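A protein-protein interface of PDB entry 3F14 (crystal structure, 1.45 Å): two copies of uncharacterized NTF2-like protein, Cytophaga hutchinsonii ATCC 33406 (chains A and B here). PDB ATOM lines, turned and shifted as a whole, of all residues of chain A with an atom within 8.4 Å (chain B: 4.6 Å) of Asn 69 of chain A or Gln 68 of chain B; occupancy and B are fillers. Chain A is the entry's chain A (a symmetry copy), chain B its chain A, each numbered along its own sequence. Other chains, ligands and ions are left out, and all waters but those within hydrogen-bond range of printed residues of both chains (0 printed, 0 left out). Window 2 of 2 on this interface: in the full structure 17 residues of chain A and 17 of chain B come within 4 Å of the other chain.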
ATOM      1  N   MET A   2      -4.116  21.329 -24.152  1.00  0.00           N
ATOM      2  CA  MET A   2      -4.744  20.529 -23.108  1.00  0.00           C
ATOM      3  C   MET A   2      -4.234  20.907 -21.715  1.00  0.00           C
ATOM      4  O   MET A   2      -5.022  21.081 -20.773  1.00  0.00           O
ATOM      5  CB  MET A   2      -4.485  19.043 -23.371  1.00  0.00           C
ATOM      6  CG  MET A   2      -5.347  18.091 -22.553  1.00  0.00           C
ATOM      7  SD  MET A   2      -7.203  17.956 -23.212  1.00  0.00           S
ATOM      8  CE  MET A   2      -7.899  19.575 -22.609  1.00  0.00           C
ATOM      9  N   GLU A   3      -2.919  21.083 -21.597  1.00  0.00           N
ATOM     10  CA  GLU A   3      -2.313  21.424 -20.322  1.00  0.00           C
ATOM     11  C   GLU A   3      -2.941  22.682 -19.723  1.00  0.00           C
ATOM     12  O   GLU A   3      -3.272  22.709 -18.535  1.00  0.00           O
ATOM     13  CB  GLU A   3      -0.793  21.598 -20.462  1.00  0.00           C
ATOM     14  N   THR A   4      -3.139  23.716 -20.539  1.00  0.00           N
ATOM     15  CA  THR A   4      -3.697  24.984 -20.014  1.00  0.00           C
ATOM     16  C   THR A   4      -5.198  24.849 -19.637  1.00  0.00           C
ATOM     17  O   THR A   4      -5.689  25.485 -18.690  1.00  0.00           O
ATOM     18  CB  THR A   4      -3.492  26.119 -21.014  1.00  0.00           C
ATOM     19  OG1 THR A   4      -4.205  25.814 -22.210  1.00  0.00           O
ATOM     20  CG2 THR A   4      -2.009  26.270 -21.341  1.00  0.00           C
ATOM     21  N   HIS A   6      -6.742  21.932 -18.630  1.00  0.00           N
ATOM     22  CA  HIS A   6      -6.704  21.221 -17.333  1.00  0.00           C
ATOM     23  C   HIS A   6      -6.364  22.152 -16.168  1.00  0.00           C
ATOM     24  O   HIS A   6      -7.011  22.111 -15.117  1.00  0.00           O
ATOM     25  CB  HIS A   6      -5.662  20.100 -17.330  1.00  0.00           C
ATOM     26  CG  HIS A   6      -5.994  18.928 -18.203  1.00  0.00           C
ATOM     27  ND1 HIS A   6      -5.089  17.914 -18.460  1.00  0.00           N
ATOM     28  CD2 HIS A   6      -7.121  18.607 -18.879  1.00  0.00           C
ATOM     29  CE1 HIS A   6      -5.660  17.007 -19.239  1.00  0.00           C
ATOM     30  NE2 HIS A   6      -6.890  17.404 -19.505  1.00  0.00           N
ATOM     31  N   TYR A   7      -5.328  22.961 -16.342  1.00  0.00           N
ATOM     32  CA  TYR A   7      -4.896  23.918 -15.325  1.00  0.00           C
ATOM     33  C   TYR A   7      -6.052  24.822 -14.910  1.00  0.00           C
ATOM     34  O   TYR A   7      -6.297  25.031 -13.736  1.00  0.00           O
ATOM     35  CB  TYR A   7      -3.727  24.753 -15.863  1.00  0.00           C
ATOM     36  CG  TYR A   7      -2.994  25.602 -14.857  1.00  0.00           C
ATOM     37  CD1 TYR A   7      -3.451  26.874 -14.509  1.00  0.00           C
ATOM     38  CD2 TYR A   7      -1.811  25.146 -14.275  1.00  0.00           C
ATOM     39  CE1 TYR A   7      -2.753  27.659 -13.583  1.00  0.00           C
ATOM     40  CE2 TYR A   7      -1.107  25.917 -13.366  1.00  0.00           C
ATOM     41  CZ  TYR A   7      -1.581  27.170 -13.016  1.00  0.00           C
ATOM     42  OH  TYR A   7      -0.875  27.925 -12.112  1.00  0.00           O
ATOM     43  N   VAL A  66       0.988  23.962  -7.570  1.00  0.00           N
ATOM     44  CA  VAL A  66       0.402  23.110  -8.568  1.00  0.00           C
ATOM     45  C   VAL A  66       1.460  22.123  -9.057  1.00  0.00           C
ATOM     46  O   VAL A  66       2.606  22.507  -9.343  1.00  0.00           O
ATOM     47  CB  VAL A  66      -0.048  23.895  -9.823  1.00  0.00           C
ATOM     48  CG1 VAL A  66      -0.610  22.921 -10.919  1.00  0.00           C
ATOM     49  CG2 VAL A  66      -1.042  24.972  -9.491  1.00  0.00           C
ATOM     50  N   ILE A  67       1.064  20.871  -9.218  1.00  0.00           N
ATOM     51  CA  ILE A  67       1.877  19.840  -9.801  1.00  0.00           C
ATOM     52  C   ILE A  67       1.096  19.175 -10.913  1.00  0.00           C
ATOM     53  O   ILE A  67       0.089  18.459 -10.668  1.00  0.00           O
ATOM     54  CB  ILE A  67       2.194  18.773  -8.785  1.00  0.00           C
ATOM     55  CG1 ILE A  67       2.857  19.410  -7.569  1.00  0.00           C
ATOM     56  CG2 ILE A  67       3.037  17.688  -9.407  1.00  0.00           C
ATOM     57  CD1 ILE A  67       3.266  18.408  -6.591  1.00  0.00           C
ATOM     58  N   GLN A  68       1.629  19.300 -12.118  1.00  0.00           N
ATOM     59  CA  GLN A  68       0.913  18.867 -13.305  1.00  0.00           C
ATOM     60  C   GLN A  68       1.746  17.891 -14.154  1.00  0.00           C
ATOM     61  O   GLN A  68       2.938  18.156 -14.372  1.00  0.00           O
ATOM     62  CB  GLN A  68       0.593  20.123 -14.140  1.00  0.00           C
ATOM     63  CG  GLN A  68      -0.287  19.874 -15.348  1.00  0.00           C
ATOM     64  CD  GLN A  68      -0.853  21.160 -15.977  1.00  0.00           C
ATOM     65  OE1 GLN A  68      -0.402  22.288 -15.701  1.00  0.00           O
ATOM     66  NE2 GLN A  68      -1.863  20.979 -16.833  1.00  0.00           N
ATOM     67  N   ASN A  69       1.134  16.799 -14.603  1.00  0.00           N
ATOM     68  CA  ASN A  69       1.717  15.947 -15.637  1.00  0.00           C
ATOM     69  C   ASN A  69       0.778  16.132 -16.862  1.00  0.00           C
ATOM     70  O   ASN A  69      -0.011  17.091 -16.904  1.00  0.00           O
ATOM     71  CB  ASN A  69       1.789  14.486 -15.179  1.00  0.00           C
ATOM     72  CG  ASN A  69       0.447  13.860 -15.163  1.00  0.00           C
ATOM     73  OD1 ASN A  69      -0.409  14.370 -15.830  1.00  0.00           O
ATOM     74  ND2 ASN A  69       0.220  12.795 -14.381  1.00  0.00           N
ATOM     75  N   GLU A  70       0.865  15.267 -17.863  1.00  0.00           N
ATOM     76  CA  GLU A  70      -0.070  15.345 -19.000  1.00  0.00           C
ATOM     77  C   GLU A  70      -1.570  15.005 -18.761  1.00  0.00           C
ATOM     78  O   GLU A  70      -2.448  15.475 -19.484  1.00  0.00           O
ATOM     79  CB  GLU A  70       0.495  14.489 -20.164  1.00  0.00           C
ATOM     80  N   ASN A  71      -1.817  14.215 -17.729  1.00  0.00           N
ATOM     81  CA  ASN A  71      -3.067  13.577 -17.334  1.00  0.00           C
ATOM     82  C   ASN A  71      -3.735  14.003 -15.973  1.00  0.00           C
ATOM     83  O   ASN A  71      -4.963  13.936 -15.757  1.00  0.00           O
ATOM     84  CB  ASN A  71      -2.558  12.129 -17.197  1.00  0.00           C
ATOM     85  CG  ASN A  71      -3.608  11.159 -16.772  1.00  0.00           C
ATOM     86  OD1 ASN A  71      -4.781  11.295 -17.131  1.00  0.00           O
ATOM     87  ND2 ASN A  71      -3.189  10.127 -16.026  1.00  0.00           N
ATOM     88  N   GLN A  72      -2.883  14.071 -14.958  1.00  0.00           N
ATOM     89  CA  GLN A  72      -3.307  14.307 -13.584  1.00  0.00           C
ATOM     90  C   GLN A  72      -2.704  15.619 -13.142  1.00  0.00           C
ATOM     91  O   GLN A  72      -1.633  16.006 -13.573  1.00  0.00           O
ATOM     92  CB  GLN A  72      -2.881  13.189 -12.599  1.00  0.00           C
ATOM     93  CG  GLN A  72      -3.484  11.790 -12.768  1.00  0.00           C
ATOM     94  CD  GLN A  72      -3.322  10.892 -11.525  1.00  0.00           C
ATOM     95  OE1 GLN A  72      -3.966  11.113 -10.481  1.00  0.00           O
ATOM     96  NE2 GLN A  72      -2.466   9.884 -11.627  1.00  0.00           N
ATOM     97  N   ILE A  73      -3.407  16.324 -12.249  1.00  0.00           N
ATOM     98  CA  ILE A  73      -2.952  17.611 -11.697  1.00  0.00           C
ATOM     99  C   ILE A  73      -3.295  17.712 -10.193  1.00  0.00           C
ATOM    100  O   ILE A  73      -4.356  17.231  -9.761  1.00  0.00           O
ATOM    101  CB  ILE A  73      -3.476  18.843 -12.531  1.00  0.00           C
ATOM    102  CG1 ILE A  73      -2.845  20.167 -12.046  1.00  0.00           C
ATOM    103  CG2 ILE A  73      -4.986  18.934 -12.513  1.00  0.00           C
ATOM    104  CD1 ILE A  73      -3.238  21.429 -12.865  1.00  0.00           C
ATOM    105  N   VAL A  74      -2.391  18.300  -9.388  1.00  0.00           N
ATOM    106  CA  VAL A  74      -2.524  18.404  -7.939  1.00  0.00           C
ATOM    107  C   VAL A  74      -2.443  19.878  -7.561  1.00  0.00           C
ATOM    108  O   VAL A  74      -1.492  20.549  -7.997  1.00  0.00           O
ATOM    109  CB  VAL A  74      -1.417  17.602  -7.229  1.00  0.00           C
ATOM    110  CG1 VAL A  74      -1.549  17.728  -5.704  1.00  0.00           C
ATOM    111  CG2 VAL A  74      -1.404  16.104  -7.694  1.00  0.00           C
ATOM    112  N   TYR A  97      -6.663  15.784  -9.376  1.00  0.00           N
ATOM    113  CA  TYR A  97      -7.566  15.578 -10.501  1.00  0.00           C
ATOM    114  C   TYR A  97      -6.996  14.579 -11.454  1.00  0.00           C
ATOM    115  O   TYR A  97      -5.826  14.675 -11.817  1.00  0.00           O
ATOM    116  CB  TYR A  97      -7.783  16.910 -11.257  1.00  0.00           C
ATOM    117  CG  TYR A  97      -8.350  18.040 -10.417  1.00  0.00           C
ATOM    118  CD1 TYR A  97      -7.525  18.799  -9.588  1.00  0.00           C
ATOM    119  CD2 TYR A  97      -9.702  18.351 -10.427  1.00  0.00           C
ATOM    120  CE1 TYR A  97      -8.006  19.784  -8.778  1.00  0.00           C
ATOM    121  CE2 TYR A  97     -10.199  19.332  -9.630  1.00  0.00           C
ATOM    122  CZ  TYR A  97      -9.351  20.076  -8.815  1.00  0.00           C
ATOM    123  OH  TYR A  97      -9.856  21.032  -7.983  1.00  0.00           O
ATOM    124  N   ARG A  98      -7.806  13.628 -11.871  1.00  0.00           N
ATOM    125  CA  ARG A  98      -7.439  12.750 -12.976  1.00  0.00           C
ATOM    126  C   ARG A  98      -8.399  13.054 -14.089  1.00  0.00           C
ATOM    127  O   ARG A  98      -9.621  12.966 -13.936  1.00  0.00           O
ATOM    128  CB  ARG A  98      -7.553  11.283 -12.618  1.00  0.00           C
ATOM    129  CG  ARG A  98      -7.117  10.331 -13.776  1.00  0.00           C
ATOM    130  CD  ARG A  98      -7.247   8.834 -13.455  1.00  0.00           C
ATOM    131  N   PHE A  99      -7.837  13.419 -15.238  1.00  0.00           N
ATOM    132  CA  PHE A  99      -8.604  13.734 -16.376  1.00  0.00           C
ATOM    133  C   PHE A  99      -8.690  12.539 -17.335  1.00  0.00           C
ATOM    134  O   PHE A  99      -7.864  11.610 -17.292  1.00  0.00           O
ATOM    135  CB  PHE A  99      -7.982  14.921 -17.131  1.00  0.00           C
ATOM    136  CG  PHE A  99      -7.951  16.174 -16.325  1.00  0.00           C
ATOM    137  CD1 PHE A  99      -9.015  17.042 -16.340  1.00  0.00           C
ATOM    138  CD2 PHE A  99      -6.841  16.478 -15.561  1.00  0.00           C
ATOM    139  CE1 PHE A  99      -8.977  18.196 -15.567  1.00  0.00           C
ATOM    140  CE2 PHE A  99      -6.804  17.603 -14.821  1.00  0.00           C
ATOM    141  CZ  PHE A  99      -7.886  18.451 -14.811  1.00  0.00           C
ATOM    142  N   GLU B   3      14.063  10.191 -13.050  1.00  0.00           N
ATOM    143  CA  GLU B   3      12.678   9.858 -12.767  1.00  0.00           C
ATOM    144  C   GLU B   3      12.570   8.607 -11.895  1.00  0.00           C
ATOM    145  O   GLU B   3      11.818   8.591 -10.917  1.00  0.00           O
ATOM    146  CB  GLU B   3      11.877   9.677 -14.065  1.00  0.00           C
ATOM    147  N   HIS B   6      13.978   9.381  -8.204  1.00  0.00           N
ATOM    148  CA  HIS B   6      12.921  10.102  -7.462  1.00  0.00           C
ATOM    149  C   HIS B   6      11.781   9.179  -7.028  1.00  0.00           C
ATOM    150  O   HIS B   6      11.328   9.231  -5.880  1.00  0.00           O
ATOM    151  CB  HIS B   6      12.298  11.219  -8.303  1.00  0.00           C
ATOM    152  CG  HIS B   6      13.200  12.386  -8.570  1.00  0.00           C
ATOM    153  ND1 HIS B   6      12.867  13.394  -9.458  1.00  0.00           N
ATOM    154  CD2 HIS B   6      14.418  12.706  -8.077  1.00  0.00           C
ATOM    155  CE1 HIS B   6      13.836  14.297  -9.475  1.00  0.00           C
ATOM    156  NE2 HIS B   6      14.785  13.902  -8.647  1.00  0.00           N
ATOM    157  N   TYR B   7      11.296   8.365  -7.955  1.00  0.00           N
ATOM    158  CA  TYR B   7      10.219   7.414  -7.683  1.00  0.00           C
ATOM    159  C   TYR B   7      10.576   6.518  -6.502  1.00  0.00           C
ATOM    160  O   TYR B   7       9.784   6.320  -5.601  1.00  0.00           O
ATOM    161  CB  TYR B   7       9.945   6.570  -8.934  1.00  0.00           C
ATOM    162  CG  TYR B   7       8.697   5.727  -8.910  1.00  0.00           C
ATOM    163  CD1 TYR B   7       8.687   4.459  -8.326  1.00  0.00           C
ATOM    164  CD2 TYR B   7       7.523   6.182  -9.511  1.00  0.00           C
ATOM    165  CE1 TYR B   7       7.525   3.679  -8.323  1.00  0.00           C
ATOM    166  CE2 TYR B   7       6.370   5.415  -9.523  1.00  0.00           C
ATOM    167  CZ  TYR B   7       6.370   4.168  -8.924  1.00  0.00           C
ATOM    168  OH  TYR B   7       5.220   3.417  -8.941  1.00  0.00           O
ATOM    169  N   VAL B  66       0.484   7.409  -7.739  1.00  0.00           N
ATOM    170  CA  VAL B  66       1.637   8.255  -7.876  1.00  0.00           C
ATOM    171  C   VAL B  66       1.398   9.235  -9.023  1.00  0.00           C
ATOM    172  O   VAL B  66       0.938   8.844 -10.108  1.00  0.00           O
ATOM    173  CB  VAL B  66       2.908   7.462  -8.261  1.00  0.00           C
ATOM    174  CG1 VAL B  66       4.127   8.430  -8.477  1.00  0.00           C
ATOM    175  CG2 VAL B  66       3.235   6.391  -7.258  1.00  0.00           C
ATOM    176  N   ILE B  67       1.770  10.486  -8.813  1.00  0.00           N
ATOM    177  CA  ILE B  67       1.752  11.509  -9.822  1.00  0.00           C
ATOM    178  C   ILE B  67       3.114  12.169  -9.869  1.00  0.00           C
ATOM    179  O   ILE B  67       3.524  12.890  -8.921  1.00  0.00           O
ATOM    180  CB  ILE B  67       0.754  12.583  -9.474  1.00  0.00           C
ATOM    181  CG1 ILE B  67      -0.620  11.953  -9.270  1.00  0.00           C
ATOM    182  CG2 ILE B  67       0.750  13.660 -10.530  1.00  0.00           C
ATOM    183  CD1 ILE B  67      -1.643  12.961  -9.019  1.00  0.00           C
ATOM    184  N   GLN B  68       3.757  12.032 -11.016  1.00  0.00           N
ATOM    185  CA  GLN B  68       5.139  12.458 -11.160  1.00  0.00           C
ATOM    186  C   GLN B  68       5.322  13.424 -12.342  1.00  0.00           C
ATOM    187  O   GLN B  68       4.780  13.152 -13.426  1.00  0.00           O
ATOM    188  CB  GLN B  68       5.993  11.197 -11.395  1.00  0.00           C
ATOM    189  CG  GLN B  68       7.489  11.439 -11.416  1.00  0.00           C
ATOM    190  CD  GLN B  68       8.326  10.150 -11.330  1.00  0.00           C
ATOM    191  OE1 GLN B  68       7.831   9.024 -11.517  1.00  0.00           O
ATOM    192  NE2 GLN B  68       9.618  10.329 -11.037  1.00  0.00           N
ATOM    193  N   ASN B  69       6.053  14.514 -12.132  1.00  0.00           N
ATOM    194  CA  ASN B  69       6.534  15.356 -13.225  1.00  0.00           C
ATOM    195  C   ASN B  69       8.076  15.165 -13.208  1.00  0.00           C
ATOM    196  O   ASN B  69       8.579  14.209 -12.593  1.00  0.00           O
ATOM    197  CB  ASN B  69       6.130  16.820 -13.020  1.00  0.00           C
ATOM    198  CG  ASN B  69       6.925  17.452 -11.941  1.00  0.00           C
ATOM    199  OD1 ASN B  69       7.970  16.940 -11.653  1.00  0.00           O
ATOM    200  ND2 ASN B  69       6.439  18.524 -11.299  1.00  0.00           N
ATOM    201  N   GLN B  72       8.757  17.256  -9.153  1.00  0.00           N
ATOM    202  CA  GLN B  72       7.912  17.033  -7.987  1.00  0.00           C
ATOM    203  C   GLN B  72       7.191  15.721  -8.195  1.00  0.00           C
ATOM    204  O   GLN B  72       6.891  15.326  -9.307  1.00  0.00           O
ATOM    205  CB  GLN B  72       6.872  18.157  -7.747  1.00  0.00           C
ATOM    206  CG  GLN B  72       7.376  19.557  -7.377  1.00  0.00           C
ATOM    207  CD  GLN B  72       6.286  20.464  -6.767  1.00  0.00           C
ATOM    208  OE1 GLN B  72       5.837  20.253  -5.625  1.00  0.00           O
ATOM    209  NE2 GLN B  72       5.859  21.467  -7.522  1.00  0.00           N
ATOM    210  N   ILE B  73       6.895  15.026  -7.090  1.00  0.00           N
ATOM    211  CA  ILE B  73       6.176  13.742  -7.113  1.00  0.00           C
ATOM    212  C   ILE B  73       5.178  13.655  -5.936  1.00  0.00           C
ATOM    213  O   ILE B  73       5.470  14.143  -4.831  1.00  0.00           O
ATOM    214  CB  ILE B  73       7.152  12.506  -7.184  1.00  0.00           C
ATOM    215  CG1 ILE B  73       6.380  11.184  -7.388  1.00  0.00           C
ATOM    216  CG2 ILE B  73       8.044  12.421  -5.965  1.00  0.00           C
ATOM    217  CD1 ILE B  73       7.266   9.916  -7.554  1.00  0.00           C
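Of the 17 printed residues of chain A, 6 touch a printed residue of chain B. Hydrophobic or aromatic side chains of chain A within 4 Å of the printed part of chain B: Ile 67 and Val 74. Of the 9 printed residues of chain B, 5 touch a printed residue of chain A. Among the printed residues, 9 pairs touch across the chains. Among the printed residues, no Asp or Glu carboxylate lies within 4 Å of a Lys or Arg side-chain nitrogen of the other chain.
Of the printed residues of chain B, Val 66 of chain A touches Gln 72 (3.9 Å). Printed residues of chain B within 4 Å of Gln 68 of chain A: Asn 69. Printed residues of chain B within 4 Å of Asn 69 of chain A: Ile 67 and Gln 68. Printed residues of chain B within 4 Å of Val 74 of chain A: Ile 67. Printed residues of chain A within 4 Å of Val 66 of chain B: Gln 72. Printed residues of chain A within 4 Å of Ile 67 of chain B: Asn 69 (3.98 Å), Gln 72 (3.3 Å) and Val 74 (3.4 Å). Printed residues of chain A within 4 Å of Gln 68 of chain B: Asn 69 (3.7 Å). The nearest printed residue of chain B that does not touch Asn 69 of chain A is Asn 69 of chain B (5.2 Å). The nearest printed residue of chain B that does not touch Gln 72 of chain A is Gln 68 of chain B (6.6 Å).
NE2 of Gln 68 of chain B sits at hydrogen-bond distance from O of Glu 3 of chain B (2.8 Å). The backbone carbonyl oxygen of Ile 67 of chain A sits at hydrogen-bond distance from the backbone NH of Val 74 of chain A. The backbone NH of Gln 72 of chain B is in hydrogen-bond range of the side-chain amide oxygen of Asn 69 of chain B (2.6 Å). The side-chain amide nitrogen of Gln 68 of chain A is in hydrogen-bond range of the backbone carbonyl oxygen of Glu 3 of chain A, at 2.8 Å. OD1 of Asn 69 of chain A lies within hydrogen-bond range of N of Gln 72 of chain A, 2.6 Å away.
Among the printed residues, pairs that only touch across the chains: Ile 67 of chain A with Gln 72 of chain B (3.3 Å), Gln 72 of chain A with Ile 67 of chain B (3.3 Å), Val 74 of chain A with Ile 67 of chain B (3.4 Å), Asn 69 of chain A with Gln 68 of chain B (3.7 Å), Gln 68 of chain A with Asn 69 of chain B (3.7 Å), Gln 72 of chain A with Val 66 of chain B (3.9 Å), Val 66 of chain A with Gln 72 of chain B (3.9 Å), Ile 67 of chain A with Asn 69 of chain B (3.98 Å) and Asn 69 of chain A with Ile 67 of chain B (3.98 Å).
Val 66 of chain A touches Gln 72 of chain B, and with the chains exchanged Gln 72 of chain A touches Val 66 of chain B. Ile 67 of chain A touches Asn 69 of chain B, and with the chains exchanged Asn 69 of chain A touches Ile 67 of chain B. Ile 67 of chain A touches Gln 72 of chain B, and with the chains exchanged Gln 72 of chain A touches Ile 67 of chain B. Gln 68 of chain A touches Asn 69 of chain B, and with the chains exchanged Asn 69 of chain A touches Gln 68 of chain B. Positions printed for both chains: 3, 6, 7, 66, 67, 68, 69, 72 and 73. Of the 9 pairs that touch across the chains among the printed residues, 8 have their exchanged pair printed and touching as well.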
